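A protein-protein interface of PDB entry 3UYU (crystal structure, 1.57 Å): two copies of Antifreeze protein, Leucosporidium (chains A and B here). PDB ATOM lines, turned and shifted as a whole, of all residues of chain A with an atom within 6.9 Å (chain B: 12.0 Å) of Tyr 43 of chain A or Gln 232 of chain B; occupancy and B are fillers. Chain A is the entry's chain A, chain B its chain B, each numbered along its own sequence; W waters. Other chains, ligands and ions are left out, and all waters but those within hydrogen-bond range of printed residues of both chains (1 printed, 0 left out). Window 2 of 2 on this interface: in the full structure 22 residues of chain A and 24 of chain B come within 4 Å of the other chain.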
ATOM      1  N   LYS A  19     -15.333  13.413  -6.339  1.00  0.00           N
ATOM      2  CA  LYS A  19     -14.244  12.889  -7.213  1.00  0.00           C
ATOM      3  C   LYS A  19     -12.944  13.639  -7.065  1.00  0.00           C
ATOM      4  O   LYS A  19     -11.869  13.063  -7.295  1.00  0.00           O
ATOM      5  CB  LYS A  19     -14.715  12.924  -8.674  1.00  0.00           C
ATOM      6  CG  LYS A  19     -15.804  11.836  -8.976  1.00  0.00           C
ATOM      7  CD  LYS A  19     -16.115  11.726 -10.461  1.00  0.00           C
ATOM      8  CE  LYS A  19     -15.016  10.953 -11.111  1.00  0.00           C
ATOM      9  NZ  LYS A  19     -15.512  10.803 -12.561  1.00  0.00           N
ATOM     10  N   ALA A  20     -13.016  14.921  -6.724  1.00  0.00           N
ATOM     11  CA  ALA A  20     -11.841  15.795  -6.764  1.00  0.00           C
ATOM     12  C   ALA A  20     -11.325  16.222  -5.405  1.00  0.00           C
ATOM     13  O   ALA A  20     -10.164  16.512  -5.240  1.00  0.00           O
ATOM     14  CB  ALA A  20     -12.150  17.045  -7.577  1.00  0.00           C
ATOM     15  N   GLY A  21     -12.215  16.259  -4.415  1.00  0.00           N
ATOM     16  CA  GLY A  21     -11.822  16.668  -3.067  1.00  0.00           C
ATOM     17  C   GLY A  21     -12.974  17.064  -2.163  1.00  0.00           C
ATOM     18  O   GLY A  21     -14.094  17.278  -2.653  1.00  0.00           O
ATOM     19  N   ILE A  22     -12.661  17.106  -0.869  1.00  0.00           N
ATOM     20  CA  ILE A  22     -13.634  17.633   0.128  1.00  0.00           C
ATOM     21  C   ILE A  22     -12.850  18.519   1.046  1.00  0.00           C
ATOM     22  O   ILE A  22     -11.817  18.084   1.561  1.00  0.00           O
ATOM     23  CB  ILE A  22     -14.296  16.503   0.907  1.00  0.00           C
ATOM     24  CG1 ILE A  22     -15.077  15.539  -0.038  1.00  0.00           C
ATOM     25  CG2 ILE A  22     -15.337  17.060   2.040  1.00  0.00           C
ATOM     26  CD1 ILE A  22     -15.413  14.198   0.699  1.00  0.00           C
ATOM     27  N   SER A  23     -13.323  19.766   1.288  1.00  0.00           N
ATOM     28  CA  SER A  23     -12.613  20.646   2.245  1.00  0.00           C
ATOM     29  C   SER A  23     -13.562  21.028   3.379  1.00  0.00           C
ATOM     30  O   SER A  23     -14.780  20.988   3.160  1.00  0.00           O
ATOM     31  CB  SER A  23     -12.198  21.960   1.560  1.00  0.00           C
ATOM     32  OG  SER A  23     -13.287  22.645   0.946  1.00  0.00           O
ATOM     33  N   VAL A  36     -13.381  10.132  -1.272  1.00  0.00           N
ATOM     34  CA  VAL A  36     -12.934  10.701  -2.530  1.00  0.00           C
ATOM     35  C   VAL A  36     -12.266   9.669  -3.409  1.00  0.00           C
ATOM     36  O   VAL A  36     -11.510   8.840  -2.873  1.00  0.00           O
ATOM     37  CB  VAL A  36     -11.990  11.937  -2.380  1.00  0.00           C
ATOM     38  CG1 VAL A  36     -12.708  13.073  -1.595  1.00  0.00           C
ATOM     39  CG2 VAL A  36     -10.733  11.581  -1.713  1.00  0.00           C
ATOM     40  N   PRO A  38     -11.370   9.646  -8.001  1.00  0.00           N
ATOM     41  CA  PRO A  38     -10.016   9.075  -7.931  1.00  0.00           C
ATOM     42  C   PRO A  38      -8.957   9.866  -7.153  1.00  0.00           C
ATOM     43  O   PRO A  38      -7.770   9.464  -7.058  1.00  0.00           O
ATOM     44  CB  PRO A  38      -9.634   9.015  -9.427  1.00  0.00           C
ATOM     45  CG  PRO A  38     -10.281  10.178  -9.994  1.00  0.00           C
ATOM     46  CD  PRO A  38     -11.691  10.094  -9.360  1.00  0.00           C
ATOM     47  N   ALA A  39      -9.396  10.996  -6.588  1.00  0.00           N
ATOM     48  CA  ALA A  39      -8.430  11.786  -5.770  1.00  0.00           C
ATOM     49  C   ALA A  39      -7.783  11.069  -4.615  1.00  0.00           C
ATOM     50  O   ALA A  39      -8.394  10.225  -3.891  1.00  0.00           O
ATOM     51  CB  ALA A  39      -9.109  13.091  -5.228  1.00  0.00           C
ATOM     52  N   ALA A  40      -6.517  11.405  -4.341  1.00  0.00           N
ATOM     53  CA  ALA A  40      -5.832  10.904  -3.160  1.00  0.00           C
ATOM     54  C   ALA A  40      -6.252  11.688  -1.844  1.00  0.00           C
ATOM     55  O   ALA A  40      -6.878  12.759  -1.952  1.00  0.00           O
ATOM     56  CB  ALA A  40      -4.289  11.119  -3.342  1.00  0.00           C
ATOM     57  N   ALA A  41      -5.864  11.167  -0.682  1.00  0.00           N
ATOM     58  CA  ALA A  41      -6.294  11.722   0.605  1.00  0.00           C
ATOM     59  C   ALA A  41      -5.789  13.147   0.787  1.00  0.00           C
ATOM     60  O   ALA A  41      -6.375  13.920   1.539  1.00  0.00           O
ATOM     61  CB  ALA A  41      -5.899  10.857   1.710  1.00  0.00           C
ATOM     62  N   THR A  42      -4.784  13.538   0.012  1.00  0.00           N
ATOM     63  CA  THR A  42      -4.315  14.911   0.092  1.00  0.00           C
ATOM     64  C   THR A  42      -5.360  15.951  -0.363  1.00  0.00           C
ATOM     65  O   THR A  42      -5.270  17.137  -0.053  1.00  0.00           O
ATOM     66  CB  THR A  42      -2.964  15.021  -0.735  1.00  0.00           C
ATOM     67  OG1 THR A  42      -2.543  16.388  -0.773  1.00  0.00           O
ATOM     68  CG2 THR A  42      -3.168  14.657  -2.101  1.00  0.00           C
ATOM     69  N   TYR A  43      -6.418  15.514  -1.047  1.00  0.00           N
ATOM     70  CA  TYR A  43      -7.454  16.422  -1.469  1.00  0.00           C
ATOM     71  C   TYR A  43      -8.656  16.461  -0.489  1.00  0.00           C
ATOM     72  O   TYR A  43      -9.645  17.122  -0.837  1.00  0.00           O
ATOM     73  CB  TYR A  43      -7.972  15.981  -2.843  1.00  0.00           C
ATOM     74  CG  TYR A  43      -6.980  16.234  -3.950  1.00  0.00           C
ATOM     75  CD1 TYR A  43      -6.826  17.503  -4.460  1.00  0.00           C
ATOM     76  CD2 TYR A  43      -6.161  15.208  -4.418  1.00  0.00           C
ATOM     77  CE1 TYR A  43      -5.921  17.759  -5.497  1.00  0.00           C
ATOM     78  CE2 TYR A  43      -5.231  15.455  -5.452  1.00  0.00           C
ATOM     79  CZ  TYR A  43      -5.143  16.717  -5.981  1.00  0.00           C
ATOM     80  OH  TYR A  43      -4.258  16.965  -7.006  1.00  0.00           O
ATOM     81  N   ILE A  44      -8.509  15.783   0.635  1.00  0.00           N
ATOM     82  CA  ILE A  44      -9.435  15.941   1.799  1.00  0.00           C
ATOM     83  C   ILE A  44      -8.718  16.840   2.817  1.00  0.00           C
ATOM     84  O   ILE A  44      -7.738  16.424   3.427  1.00  0.00           O
ATOM     85  CB  ILE A  44      -9.786  14.604   2.409  1.00  0.00           C
ATOM     86  CG1 ILE A  44     -10.498  13.688   1.373  1.00  0.00           C
ATOM     87  CG2 ILE A  44     -10.654  14.792   3.727  1.00  0.00           C
ATOM     88  CD1 ILE A  44     -10.733  12.186   1.944  1.00  0.00           C
ATOM     89  N   THR A  45      -9.226  18.064   2.976  1.00  0.00           N
ATOM     90  CA  THR A  45      -8.493  19.133   3.679  1.00  0.00           C
ATOM     91  C   THR A  45      -9.377  19.687   4.794  1.00  0.00           C
ATOM     92  O   THR A  45     -10.609  19.810   4.621  1.00  0.00           O
ATOM     93  CB  THR A  45      -8.045  20.317   2.730  1.00  0.00           C
ATOM     94  OG1 THR A  45      -9.153  20.922   2.066  1.00  0.00           O
ATOM     95  CG2 THR A  45      -7.034  19.815   1.654  1.00  0.00           C
ATOM     96  N   ASP A  71      -6.127   6.396  -2.567  1.00  0.00           N
ATOM     97  CA  ASP A  71      -4.768   5.838  -2.313  1.00  0.00           C
ATOM     98  C   ASP A  71      -4.651   4.970  -1.071  1.00  0.00           C
ATOM     99  O   ASP A  71      -3.550   4.477  -0.712  1.00  0.00           O
ATOM    100  CB  ASP A  71      -3.701   6.961  -2.287  1.00  0.00           C
ATOM    101  CG  ASP A  71      -3.999   8.065  -1.248  1.00  0.00           C
ATOM    102  OD1 ASP A  71      -5.195   8.443  -1.036  1.00  0.00           O
ATOM    103  OD2 ASP A  71      -3.037   8.647  -0.692  1.00  0.00           O
ATOM    104  N   GLU A 212     -15.787  18.754  -6.584  1.00  0.00           N
ATOM    105  CA  GLU A 212     -15.365  19.074  -5.191  1.00  0.00           C
ATOM    106  C   GLU A 212     -16.550  19.487  -4.306  1.00  0.00           C
ATOM    107  O   GLU A 212     -17.515  20.098  -4.782  1.00  0.00           O
ATOM    108  CB  GLU A 212     -14.390  20.291  -5.291  1.00  0.00           C
ATOM    109  CG  GLU A 212     -13.913  20.870  -3.976  1.00  0.00           C
ATOM    110  CD  GLU A 212     -12.622  20.236  -3.462  1.00  0.00           C
ATOM    111  OE1 GLU A 212     -11.975  19.532  -4.281  1.00  0.00           O
ATOM    112  OE2 GLU A 212     -12.242  20.456  -2.264  1.00  0.00           O
ATOM    113  N   VAL A 213     -16.409  19.164  -3.038  1.00  0.00           N
ATOM    114  CA  VAL A 213     -17.385  19.609  -1.990  1.00  0.00           C
ATOM    115  C   VAL A 213     -16.665  20.470  -0.969  1.00  0.00           C
ATOM    116  O   VAL A 213     -15.630  20.068  -0.423  1.00  0.00           O
ATOM    117  CB  VAL A 213     -18.060  18.388  -1.298  1.00  0.00           C
ATOM    118  CG1 VAL A 213     -18.965  18.857  -0.094  1.00  0.00           C
ATOM    119  CG2 VAL A 213     -18.830  17.587  -2.325  1.00  0.00           C
ATOM    120  N   PRO B 228      -9.378   2.490 -10.530  1.00  0.00           N
ATOM    121  CA  PRO B 228      -9.139   3.813 -11.124  1.00  0.00           C
ATOM    122  C   PRO B 228      -7.720   4.338 -10.839  1.00  0.00           C
ATOM    123  O   PRO B 228      -7.160   4.092  -9.759  1.00  0.00           O
ATOM    124  CB  PRO B 228     -10.167   4.702 -10.394  1.00  0.00           C
ATOM    125  CG  PRO B 228     -11.309   3.761 -10.070  1.00  0.00           C
ATOM    126  CD  PRO B 228     -10.630   2.462  -9.733  1.00  0.00           C
ATOM    127  N   GLU B 229      -7.106   5.037 -11.802  1.00  0.00           N
ATOM    128  CA  GLU B 229      -5.794   5.608 -11.520  1.00  0.00           C
ATOM    129  C   GLU B 229      -5.924   6.774 -10.500  1.00  0.00           C
ATOM    130  O   GLU B 229      -6.713   7.660 -10.705  1.00  0.00           O
ATOM    131  CB  GLU B 229      -5.151   6.107 -12.826  1.00  0.00           C
ATOM    132  CG  GLU B 229      -3.730   6.620 -12.601  1.00  0.00           C
ATOM    133  CD  GLU B 229      -2.974   6.970 -13.886  1.00  0.00           C
ATOM    134  OE1 GLU B 229      -3.505   6.678 -14.997  1.00  0.00           O
ATOM    135  OE2 GLU B 229      -1.861   7.573 -13.764  1.00  0.00           O
ATOM    136  N   VAL B 230      -5.121   6.740  -9.453  1.00  0.00           N
ATOM    137  CA  VAL B 230      -5.140   7.760  -8.378  1.00  0.00           C
ATOM    138  C   VAL B 230      -4.665   9.116  -8.925  1.00  0.00           C
ATOM    139  O   VAL B 230      -3.697   9.174  -9.688  1.00  0.00           O
ATOM    140  CB  VAL B 230      -4.330   7.284  -7.117  1.00  0.00           C
ATOM    141  CG1 VAL B 230      -4.183   8.385  -5.994  1.00  0.00           C
ATOM    142  CG2 VAL B 230      -4.946   6.049  -6.533  1.00  0.00           C
ATOM    143  N   VAL B 231      -5.394  10.176  -8.611  1.00  0.00           N
ATOM    144  CA  VAL B 231      -4.996  11.558  -8.919  1.00  0.00           C
ATOM    145  C   VAL B 231      -4.242  12.125  -7.709  1.00  0.00           C
ATOM    146  O   VAL B 231      -4.815  12.280  -6.599  1.00  0.00           O
ATOM    147  CB  VAL B 231      -6.219  12.424  -9.376  1.00  0.00           C
ATOM    148  CG1 VAL B 231      -5.815  13.935  -9.532  1.00  0.00           C
ATOM    149  CG2 VAL B 231      -6.841  11.869 -10.675  1.00  0.00           C
ATOM    150  N   GLN B 232      -2.949  12.431  -7.908  1.00  0.00           N
ATOM    151  CA  GLN B 232      -2.117  13.004  -6.859  1.00  0.00           C
ATOM    152  C   GLN B 232      -1.853  14.447  -7.305  1.00  0.00           C
ATOM    153  O   GLN B 232      -1.828  15.373  -6.469  1.00  0.00           O
ATOM    154  CB  GLN B 232      -0.776  12.225  -6.686  1.00  0.00           C
ATOM    155  CG  GLN B 232      -0.844  10.741  -6.242  1.00  0.00           C
ATOM    156  CD  GLN B 232      -0.782  10.518  -4.721  1.00  0.00           C
ATOM    157  OE1 GLN B 232      -0.736  11.489  -3.919  1.00  0.00           O
ATOM    158  NE2 GLN B 232      -0.804   9.237  -4.307  1.00  0.00           N
HETATM  159  O   HOH W   1      -0.588   8.429  -1.781  1.00  0.00           O
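Tyr 43 of chain A touches just these residues of chain B: Val 231 (3.4 Å) and Gln 232 (3.0 Å).
No residue of chain B comes within 4 Å of Ile 22 of chain A.
Ala 39 of chain A touches just one residue of chain B: Val 231 (3.7 Å).
Ala 40 of chain A touches just these residues of chain B: Val 230 (3.8 Å), Val 231 (3.0 Å) and Gln 232 (3.6 Å).
No residue of chain B comes within 4 Å of Thr 42 of chain A.
No residue of chain B comes within 4 Å of Thr 45 of chain A.
Printed residues of chain B within 4 Å of Pro 38 of chain A: Glu 229, Val 230 and Val 231.
Printed residues of chain A within 4 Å of Glu 229 of chain B: Pro 38.
Of the printed residues of chain A, Val 231 of chain B touches Pro 38, Ala 39, Ala 40 and Tyr 43.
Glu 212 of chain A touches none of the printed residues of chain B.
Val 213 of chain A touches none of the printed residues of chain B.
The nearest residue of chain A that does not touch Gln 232 of chain B is Asp 71 of chain A (4.2 Å).
The nearest printed residue of chain A that does not touch Val 230 of chain B is Asp 71 of chain A (4.0002 Å).
O of Lys 19 of chain A lies within hydrogen-bond range of N of Ala 39 of chain A, at 3.3 Å.
The backbone NH of Ile 22 of chain A is in hydrogen-bond range of the backbone carbonyl oxygen of Tyr 43 of chain A (3.0 Å).
No position is printed for both chains.
Water W1 bridges the side-chain amide nitrogen (NE2) of Gln 232 of chain B (2.7 Å) and the side-chain carboxylate (OD2) of Asp 71 of chain A (2.7 Å).
The backbone carbonyl oxygen (O) of Pro 38 of chain A is in hydrogen-bond range of the backbone NH (N) of Val 231 of chain B, at 2.9 Å.
N of Ala 40 of chain A lies within hydrogen-bond range of O of Val 231 of chain B, at 3.0 Å.
O of Gln 232 of chain B lies within hydrogen-bond range of OH of Tyr 43 of chain A (3.0 Å).
Among the printed residues, merely in contact across the chains: Pro 38 of chain A with Glu 229 of chain B (3.5 Å), Pro 38 of chain A with Val 230 of chain B (3.4 Å), Ala 39 of chain A with Val 231 of chain B (3.7 Å), Ala 40 of chain A with Val 230 of chain B (3.8 Å), Ala 40 of chain A with Gln 232 of chain B (3.6 Å) and Tyr 43 of chain A with Val 231 of chain B (3.4 Å).
Printed residues of chain A that touch a printed residue of chain B: Pro 38, Ala 39, Ala 40 and Tyr 43.
Hydrophobic or aromatic side chains of chain A within 4 Å of the printed part of chain B: Pro 38, Ala 40 and Tyr 43.
Hydrophobic or aromatic side chains of chain B within 4 Å of the printed part of chain A: Val 230 and Val 231.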
